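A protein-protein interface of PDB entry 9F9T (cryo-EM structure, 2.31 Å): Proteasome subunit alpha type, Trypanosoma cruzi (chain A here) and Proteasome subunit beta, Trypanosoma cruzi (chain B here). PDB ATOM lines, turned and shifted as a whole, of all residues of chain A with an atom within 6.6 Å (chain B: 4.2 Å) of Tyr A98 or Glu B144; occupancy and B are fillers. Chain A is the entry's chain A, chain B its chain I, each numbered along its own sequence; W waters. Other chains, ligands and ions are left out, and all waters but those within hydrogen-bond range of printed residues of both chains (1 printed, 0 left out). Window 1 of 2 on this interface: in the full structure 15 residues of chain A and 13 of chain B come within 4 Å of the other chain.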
ATOM      1  N   GLN A  93      12.034  -3.424  -0.544  1.00  0.00           N
ATOM      2  CA  GLN A  93      11.313  -4.498  -1.215  1.00  0.00           C
ATOM      3  C   GLN A  93      12.159  -5.083  -2.342  1.00  0.00           C
ATOM      4  O   GLN A  93      12.200  -6.281  -2.570  1.00  0.00           O
ATOM      5  CB  GLN A  93       9.993  -3.954  -1.698  1.00  0.00           C
ATOM      6  CG  GLN A  93       9.133  -5.032  -2.256  1.00  0.00           C
ATOM      7  CD  GLN A  93       7.873  -4.470  -2.870  1.00  0.00           C
ATOM      8  OE1 GLN A  93       7.367  -3.421  -2.463  1.00  0.00           O
ATOM      9  NE2 GLN A  93       7.379  -5.170  -3.883  1.00  0.00           N
ATOM     10  N   GLU A  94      12.805  -4.193  -3.069  1.00  0.00           N
ATOM     11  CA  GLU A  94      13.781  -4.524  -4.086  1.00  0.00           C
ATOM     12  C   GLU A  94      14.935  -5.313  -3.477  1.00  0.00           C
ATOM     13  O   GLU A  94      15.440  -6.221  -4.100  1.00  0.00           O
ATOM     14  CB  GLU A  94      14.332  -3.230  -4.701  1.00  0.00           C
ATOM     15  CG  GLU A  94      14.672  -3.370  -6.161  1.00  0.00           C
ATOM     16  CD  GLU A  94      13.509  -3.573  -7.162  1.00  0.00           C
ATOM     17  OE1 GLU A  94      13.797  -3.913  -8.366  1.00  0.00           O
ATOM     18  OE2 GLU A  94      12.310  -3.383  -6.775  1.00  0.00           O
ATOM     19  N   ALA A  95      15.410  -4.901  -2.310  1.00  0.00           N
ATOM     20  CA  ALA A  95      16.553  -5.584  -1.761  1.00  0.00           C
ATOM     21  C   ALA A  95      16.186  -7.009  -1.368  1.00  0.00           C
ATOM     22  O   ALA A  95      16.987  -7.921  -1.531  1.00  0.00           O
ATOM     23  CB  ALA A  95      17.128  -4.821  -0.647  1.00  0.00           C
ATOM     24  N   SER A  96      14.989  -7.147  -0.834  1.00  0.00           N
ATOM     25  CA  SER A  96      14.490  -8.398  -0.320  1.00  0.00           C
ATOM     26  C   SER A  96      14.147  -9.363  -1.466  1.00  0.00           C
ATOM     27  O   SER A  96      14.490 -10.538  -1.385  1.00  0.00           O
ATOM     28  CB  SER A  96      13.323  -8.122   0.594  1.00  0.00           C
ATOM     29  OG  SER A  96      12.102  -8.528  -0.035  1.00  0.00           O
ATOM     30  N   GLU A  97      13.513  -8.885  -2.545  1.00  0.00           N
ATOM     31  CA  GLU A  97      13.326  -9.696  -3.732  1.00  0.00           C
ATOM     32  C   GLU A  97      14.640 -10.142  -4.365  1.00  0.00           C
ATOM     33  O   GLU A  97      14.767 -11.269  -4.809  1.00  0.00           O
ATOM     34  CB  GLU A  97      12.539  -8.952  -4.800  1.00  0.00           C
ATOM     35  CG  GLU A  97      11.036  -8.847  -4.508  1.00  0.00           C
ATOM     36  CD  GLU A  97      10.311  -7.665  -5.162  1.00  0.00           C
ATOM     37  OE1 GLU A  97      10.966  -6.973  -6.012  1.00  0.00           O
ATOM     38  OE2 GLU A  97       9.118  -7.370  -4.789  1.00  0.00           O
ATOM     39  N   TYR A  98      15.618  -9.258  -4.430  1.00  0.00           N
ATOM     40  CA  TYR A  98      16.898  -9.613  -5.013  1.00  0.00           C
ATOM     41  C   TYR A  98      17.513 -10.734  -4.210  1.00  0.00           C
ATOM     42  O   TYR A  98      18.109 -11.621  -4.761  1.00  0.00           O
ATOM     43  CB  TYR A  98      17.864  -8.443  -5.088  1.00  0.00           C
ATOM     44  CG  TYR A  98      19.249  -8.720  -5.673  1.00  0.00           C
ATOM     45  CD1 TYR A  98      19.574  -8.209  -6.925  1.00  0.00           C
ATOM     46  CD2 TYR A  98      20.267  -9.395  -4.960  1.00  0.00           C
ATOM     47  CE1 TYR A  98      20.848  -8.354  -7.449  1.00  0.00           C
ATOM     48  CE2 TYR A  98      21.539  -9.540  -5.487  1.00  0.00           C
ATOM     49  CZ  TYR A  98      21.807  -9.087  -6.773  1.00  0.00           C
ATOM     50  OH  TYR A  98      23.032  -9.208  -7.406  1.00  0.00           O
ATOM     51  N   LYS A  99      17.366 -10.695  -2.908  1.00  0.00           N
ATOM     52  CA  LYS A  99      18.051 -11.678  -2.138  1.00  0.00           C
ATOM     53  C   LYS A  99      17.373 -13.021  -2.237  1.00  0.00           C
ATOM     54  O   LYS A  99      18.040 -14.040  -2.143  1.00  0.00           O
ATOM     55  CB  LYS A  99      18.058 -11.309  -0.666  1.00  0.00           C
ATOM     56  CG  LYS A  99      18.727 -12.358   0.187  1.00  0.00           C
ATOM     57  CD  LYS A  99      19.279 -11.726   1.368  1.00  0.00           C
ATOM     58  CE  LYS A  99      19.963 -12.744   2.248  1.00  0.00           C
ATOM     59  NZ  LYS A  99      20.617 -12.011   3.374  1.00  0.00           N
ATOM     60  N   TYR A 100      16.066 -13.025  -2.393  1.00  0.00           N
ATOM     61  CA  TYR A 100      15.360 -14.279  -2.527  1.00  0.00           C
ATOM     62  C   TYR A 100      15.628 -14.871  -3.901  1.00  0.00           C
ATOM     63  O   TYR A 100      15.638 -16.069  -4.040  1.00  0.00           O
ATOM     64  CB  TYR A 100      13.861 -14.076  -2.219  1.00  0.00           C
ATOM     65  CG  TYR A 100      13.005 -15.348  -2.325  1.00  0.00           C
ATOM     66  CD1 TYR A 100      13.053 -16.316  -1.325  1.00  0.00           C
ATOM     67  CD2 TYR A 100      12.252 -15.609  -3.475  1.00  0.00           C
ATOM     68  CE1 TYR A 100      12.317 -17.482  -1.426  1.00  0.00           C
ATOM     69  CE2 TYR A 100      11.528 -16.785  -3.604  1.00  0.00           C
ATOM     70  CZ  TYR A 100      11.576 -17.733  -2.582  1.00  0.00           C
ATOM     71  OH  TYR A 100      10.852 -18.907  -2.700  1.00  0.00           O
ATOM     72  N   ARG A 101      15.924 -14.070  -4.906  1.00  0.00           N
ATOM     73  CA  ARG A 101      16.053 -14.568  -6.264  1.00  0.00           C
ATOM     74  C   ARG A 101      17.474 -15.039  -6.548  1.00  0.00           C
ATOM     75  O   ARG A 101      17.686 -15.989  -7.283  1.00  0.00           O
ATOM     76  CB  ARG A 101      15.605 -13.498  -7.251  1.00  0.00           C
ATOM     77  CG  ARG A 101      15.913 -13.851  -8.692  1.00  0.00           C
ATOM     78  CD  ARG A 101      14.791 -13.434  -9.613  1.00  0.00           C
ATOM     79  NE  ARG A 101      15.297 -13.174 -10.953  1.00  0.00           N
ATOM     80  CZ  ARG A 101      15.009 -12.092 -11.661  1.00  0.00           C
ATOM     81  NH1 ARG A 101      14.105 -11.233 -11.209  1.00  0.00           N
ATOM     82  NH2 ARG A 101      15.600 -11.892 -12.828  1.00  0.00           N
ATOM     83  N   TYR A 102      18.437 -14.404  -5.943  1.00  0.00           N
ATOM     84  CA  TYR A 102      19.802 -14.718  -6.257  1.00  0.00           C
ATOM     85  C   TYR A 102      20.510 -15.317  -5.047  1.00  0.00           C
ATOM     86  O   TYR A 102      21.648 -15.761  -5.171  1.00  0.00           O
ATOM     87  CB  TYR A 102      20.576 -13.461  -6.650  1.00  0.00           C
ATOM     88  CG  TYR A 102      20.080 -12.859  -7.929  1.00  0.00           C
ATOM     89  CD1 TYR A 102      20.125 -13.596  -9.083  1.00  0.00           C
ATOM     90  CD2 TYR A 102      19.444 -11.622  -8.000  1.00  0.00           C
ATOM     91  CE1 TYR A 102      19.601 -13.128 -10.286  1.00  0.00           C
ATOM     92  CE2 TYR A 102      19.001 -11.096  -9.206  1.00  0.00           C
ATOM     93  CZ  TYR A 102      19.092 -11.852 -10.359  1.00  0.00           C
ATOM     94  OH  TYR A 102      18.665 -11.520 -11.601  1.00  0.00           O
ATOM     95  N   GLY A 103      19.900 -15.189  -3.863  1.00  0.00           N
ATOM     96  CA  GLY A 103      20.452 -15.753  -2.638  1.00  0.00           C
ATOM     97  C   GLY A 103      21.638 -15.052  -2.001  1.00  0.00           C
ATOM     98  O   GLY A 103      22.279 -15.637  -1.144  1.00  0.00           O
ATOM     99  N   SER A 104      21.903 -13.812  -2.387  1.00  0.00           N
ATOM    100  CA  SER A 104      23.000 -13.032  -1.808  1.00  0.00           C
ATOM    101  C   SER A 104      22.458 -11.623  -1.619  1.00  0.00           C
ATOM    102  O   SER A 104      21.608 -11.224  -2.386  1.00  0.00           O
ATOM    103  CB  SER A 104      24.218 -13.001  -2.777  1.00  0.00           C
ATOM    104  OG  SER A 104      25.463 -12.943  -2.110  1.00  0.00           O
ATOM    105  N   PRO A 105      22.931 -10.782  -0.691  1.00  0.00           N
ATOM    106  CA  PRO A 105      22.402  -9.414  -0.602  1.00  0.00           C
ATOM    107  C   PRO A 105      22.730  -8.486  -1.776  1.00  0.00           C
ATOM    108  O   PRO A 105      23.851  -8.417  -2.230  1.00  0.00           O
ATOM    109  CB  PRO A 105      23.060  -8.778   0.651  1.00  0.00           C
ATOM    110  CG  PRO A 105      24.036  -9.839   1.203  1.00  0.00           C
ATOM    111  CD  PRO A 105      23.984 -11.071   0.296  1.00  0.00           C
ATOM    112  N   ILE A 106      21.768  -7.682  -2.179  1.00  0.00           N
ATOM    113  CA  ILE A 106      21.982  -6.760  -3.279  1.00  0.00           C
ATOM    114  C   ILE A 106      23.216  -5.920  -3.046  1.00  0.00           C
ATOM    115  O   ILE A 106      23.489  -5.555  -1.909  1.00  0.00           O
ATOM    116  CB  ILE A 106      20.728  -5.888  -3.526  1.00  0.00           C
ATOM    117  CG1 ILE A 106      20.729  -5.338  -4.951  1.00  0.00           C
ATOM    118  CG2 ILE A 106      20.559  -4.844  -2.458  1.00  0.00           C
ATOM    119  CD1 ILE A 106      19.401  -4.886  -5.372  1.00  0.00           C
ATOM    120  N   PRO A 107      24.117  -5.766  -4.035  1.00  0.00           N
ATOM    121  CA  PRO A 107      25.205  -4.764  -3.956  1.00  0.00           C
ATOM    122  C   PRO A 107      24.655  -3.366  -4.014  1.00  0.00           C
ATOM    123  O   PRO A 107      23.690  -3.116  -4.689  1.00  0.00           O
ATOM    124  CB  PRO A 107      26.066  -5.027  -5.175  1.00  0.00           C
ATOM    125  CG  PRO A 107      25.732  -6.524  -5.533  1.00  0.00           C
ATOM    126  CD  PRO A 107      24.304  -6.728  -5.116  1.00  0.00           C
ATOM    127  N   VAL A 110      24.040  -1.870  -7.583  1.00  0.00           N
ATOM    128  CA  VAL A 110      22.880  -2.395  -8.246  1.00  0.00           C
ATOM    129  C   VAL A 110      21.577  -1.927  -7.590  1.00  0.00           C
ATOM    130  O   VAL A 110      20.603  -1.625  -8.280  1.00  0.00           O
ATOM    131  CB  VAL A 110      22.953  -3.911  -8.193  1.00  0.00           C
ATOM    132  CG1 VAL A 110      21.673  -4.510  -8.683  1.00  0.00           C
ATOM    133  CG2 VAL A 110      24.099  -4.445  -9.015  1.00  0.00           C
ATOM    134  N   ARG A 114      18.412   0.221  -9.557  1.00  0.00           N
ATOM    135  CA  ARG A 114      17.009  -0.147  -9.536  1.00  0.00           C
ATOM    136  C   ARG A 114      16.114   0.979  -9.041  1.00  0.00           C
ATOM    137  O   ARG A 114      14.975   1.055  -9.412  1.00  0.00           O
ATOM    138  CB  ARG A 114      16.801  -1.318  -8.573  1.00  0.00           C
ATOM    139  CG  ARG A 114      17.470  -2.582  -9.051  1.00  0.00           C
ATOM    140  CD  ARG A 114      16.815  -3.143 -10.280  1.00  0.00           C
ATOM    141  NE  ARG A 114      16.995  -4.586 -10.195  1.00  0.00           N
ATOM    142  CZ  ARG A 114      18.123  -5.232 -10.490  1.00  0.00           C
ATOM    143  NH1 ARG A 114      18.251  -6.514 -10.186  1.00  0.00           N
ATOM    144  NH2 ARG A 114      19.109  -4.572 -11.083  1.00  0.00           N
ATOM    145  N   HIS B 132      22.494 -10.865 -15.772  1.00  0.00           N
ATOM    146  CA  HIS B 132      23.002 -10.410 -14.497  1.00  0.00           C
ATOM    147  C   HIS B 132      24.454  -9.931 -14.538  1.00  0.00           C
ATOM    148  O   HIS B 132      24.756  -8.923 -13.918  1.00  0.00           O
ATOM    149  CB  HIS B 132      22.743 -11.475 -13.452  1.00  0.00           C
ATOM    150  CG  HIS B 132      22.858 -10.998 -12.058  1.00  0.00           C
ATOM    151  ND1 HIS B 132      23.660 -11.644 -11.146  1.00  0.00           N
ATOM    152  CD2 HIS B 132      22.248 -10.005 -11.399  1.00  0.00           C
ATOM    153  CE1 HIS B 132      23.560 -10.995  -9.985  1.00  0.00           C
ATOM    154  NE2 HIS B 132      22.702 -10.011 -10.121  1.00  0.00           N
ATOM    155  N   ARG B 141      28.469 -15.463  -9.242  1.00  0.00           N
ATOM    156  CA  ARG B 141      28.795 -16.285  -8.084  1.00  0.00           C
ATOM    157  C   ARG B 141      28.157 -17.661  -8.199  1.00  0.00           C
ATOM    158  O   ARG B 141      27.054 -17.784  -8.685  1.00  0.00           O
ATOM    159  CB  ARG B 141      28.300 -15.593  -6.821  1.00  0.00           C
ATOM    160  CG  ARG B 141      28.688 -14.133  -6.695  1.00  0.00           C
ATOM    161  CD  ARG B 141      30.033 -13.998  -6.044  1.00  0.00           C
ATOM    162  NE  ARG B 141      30.324 -12.589  -5.713  1.00  0.00           N
ATOM    163  CZ  ARG B 141      30.638 -12.141  -4.499  1.00  0.00           C
ATOM    164  NH1 ARG B 141      31.158 -10.941  -4.373  1.00  0.00           N
ATOM    165  NH2 ARG B 141      30.555 -12.930  -3.434  1.00  0.00           N
ATOM    166  N   VAL B 142      28.890 -18.689  -7.822  1.00  0.00           N
ATOM    167  CA  VAL B 142      28.379 -20.053  -7.895  1.00  0.00           C
ATOM    168  C   VAL B 142      27.082 -20.209  -7.081  1.00  0.00           C
ATOM    169  O   VAL B 142      26.096 -20.729  -7.555  1.00  0.00           O
ATOM    170  CB  VAL B 142      29.444 -21.130  -7.540  1.00  0.00           C
ATOM    171  CG1 VAL B 142      28.979 -22.505  -7.955  1.00  0.00           C
ATOM    172  CG2 VAL B 142      30.758 -20.910  -8.256  1.00  0.00           C
ATOM    173  N   HIS B 143      27.023 -19.575  -5.924  1.00  0.00           N
ATOM    174  CA  HIS B 143      25.817 -19.570  -5.115  1.00  0.00           C
ATOM    175  C   HIS B 143      24.557 -19.023  -5.808  1.00  0.00           C
ATOM    176  O   HIS B 143      23.464 -19.489  -5.500  1.00  0.00           O
ATOM    177  CB  HIS B 143      26.152 -19.020  -3.722  1.00  0.00           C
ATOM    178  CG  HIS B 143      25.055 -19.265  -2.731  1.00  0.00           C
ATOM    179  ND1 HIS B 143      24.225 -18.243  -2.292  1.00  0.00           N
ATOM    180  CD2 HIS B 143      24.625 -20.431  -2.132  1.00  0.00           C
ATOM    181  CE1 HIS B 143      23.300 -18.782  -1.489  1.00  0.00           C
ATOM    182  NE2 HIS B 143      23.525 -20.103  -1.381  1.00  0.00           N
ATOM    183  N   GLU B 144      24.724 -18.037  -6.684  1.00  0.00           N
ATOM    184  CA  GLU B 144      23.664 -17.406  -7.463  1.00  0.00           C
ATOM    185  C   GLU B 144      23.090 -18.409  -8.444  1.00  0.00           C
ATOM    186  O   GLU B 144      21.891 -18.560  -8.516  1.00  0.00           O
ATOM    187  CB  GLU B 144      24.104 -16.095  -8.163  1.00  0.00           C
ATOM    188  CG  GLU B 144      24.608 -15.020  -7.177  1.00  0.00           C
ATOM    189  CD  GLU B 144      25.060 -13.590  -7.617  1.00  0.00           C
ATOM    190  OE1 GLU B 144      25.901 -13.411  -8.594  1.00  0.00           O
ATOM    191  OE2 GLU B 144      24.645 -12.586  -6.915  1.00  0.00           O
ATOM    192  N   ALA B 145      23.961 -19.149  -9.124  1.00  0.00           N
ATOM    193  CA  ALA B 145      23.529 -20.210 -10.008  1.00  0.00           C
ATOM    194  C   ALA B 145      22.766 -21.269  -9.242  1.00  0.00           C
ATOM    195  O   ALA B 145      21.729 -21.714  -9.714  1.00  0.00           O
ATOM    196  CB  ALA B 145      24.722 -20.817 -10.682  1.00  0.00           C
ATOM    197  N   LEU B 146      23.352 -21.741  -8.135  1.00  0.00           N
ATOM    198  CA  LEU B 146      22.765 -22.802  -7.343  1.00  0.00           C
ATOM    199  C   LEU B 146      21.343 -22.415  -6.966  1.00  0.00           C
ATOM    200  O   LEU B 146      20.409 -23.226  -7.128  1.00  0.00           O
ATOM    201  CB  LEU B 146      23.595 -23.021  -6.070  1.00  0.00           C
ATOM    202  CG  LEU B 146      23.085 -24.225  -5.253  1.00  0.00           C
ATOM    203  CD1 LEU B 146      23.091 -25.467  -6.121  1.00  0.00           C
ATOM    204  CD2 LEU B 146      23.910 -24.531  -3.970  1.00  0.00           C
ATOM    205  N   THR B 147      21.203 -21.172  -6.531  1.00  0.00           N
ATOM    206  CA  THR B 147      19.943 -20.630  -6.071  1.00  0.00           C
ATOM    207  C   THR B 147      18.924 -20.446  -7.207  1.00  0.00           C
ATOM    208  O   THR B 147      17.783 -20.833  -7.081  1.00  0.00           O
ATOM    209  CB  THR B 147      20.165 -19.320  -5.287  1.00  0.00           C
ATOM    210  OG1 THR B 147      20.900 -19.504  -4.081  1.00  0.00           O
ATOM    211  CG2 THR B 147      18.882 -18.652  -4.912  1.00  0.00           C
ATOM    212  N   MET B 148      19.296 -19.948  -8.358  1.00  0.00           N
ATOM    213  CA  MET B 148      18.332 -19.859  -9.458  1.00  0.00           C
ATOM    214  C   MET B 148      17.907 -21.256  -9.901  1.00  0.00           C
ATOM    215  O   MET B 148      16.778 -21.485 -10.317  1.00  0.00           O
ATOM    216  CB  MET B 148      18.997 -19.132 -10.612  1.00  0.00           C
ATOM    217  CG  MET B 148      19.348 -17.760 -10.185  1.00  0.00           C
ATOM    218  SD  MET B 148      20.751 -17.018 -11.094  1.00  0.00           S
ATOM    219  CE  MET B 148      19.890 -16.279 -12.486  1.00  0.00           C
HETATM  220  O   HOH W   1      23.833 -16.186  -3.894  1.00  0.00           O
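The side-chain hydroxyl of Tyr A98 sits at hydrogen-bond distance from a ring nitrogen (NE2) of His B132, at 2.9 Å. The backbone carbonyl oxygen (O) of Gly A103 lies close to a ring nitrogen (ND1) of His B143 (3.4 Å).
OH of Tyr A102 is in hydrogen-bond range of NH2 of Arg A101, 3.3 Å away. The backbone NH (N) of Arg B141 lies within hydrogen-bond range of the side-chain carboxylate (OE1) of Glu B144, at 3.4 Å. OG1 of Thr B147 is in hydrogen-bond range of O of His B143.
Of the printed residues of chain B, Arg A101 touches Thr B147 and Met B148. Of the printed residues of chain A, His B132 touches Tyr A98 and Tyr A102. Printed residues of chain A within 4 Å of His B143: Gly A103 (3.3 Å). Of the printed residues of chain A, Thr B147 touches Arg A101 (3.8 Å), Tyr A102 (3.7 Å) and Gly A103 (3.8 Å). Printed residues of chain A within 4 Å of Met B148: Arg A101 (3.8 Å) and Tyr A102 (3.9 Å). The nearest printed residue of chain B that does not touch Tyr A98 is Thr B147 (7.1 Å). The nearest residue of chain A that does not touch Glu B144 is Ser A104 (4.2 Å). The nearest printed residue of chain A that does not touch His B132 is Arg A114 (5.4 Å).
Water W1 lies within hydrogen-bond range of O of Tyr A102 (2.6 Å), ND1 of His B143 (2.6 Å), O of Gly A103 (3.2 Å), N of Ser A104 (3.4 Å) and N of Glu B144 (3.5 Å).
Among the printed residues, merely in contact across the chains: Tyr A98 with Glu B144 (3.8 Å), Arg A101 with Thr B147 (3.8 Å), Arg A101 with Met B148 (3.8 Å), Tyr A102 with His B132 (3.8 Å), Tyr A102 with Glu B144 (3.5 Å), Tyr A102 with Thr B147 (3.7 Å), Tyr A102 with Met B148 (3.9 Å) and Gly A103 with Thr B147 (3.8 Å).
Of the 17 printed residues of chain A, 4 touch a printed residue of chain B. Of the 9 printed residues of chain B, 5 touch a printed residue of chain A. Printed residues of chain B that touch a printed residue of chain A: His B132, His B143, Glu B144, Thr B147 and Met B148. Hydrophobic or aromatic side chains of chain B within 4 Å of the printed part of chain A: His B132, His B143 and Met B148.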
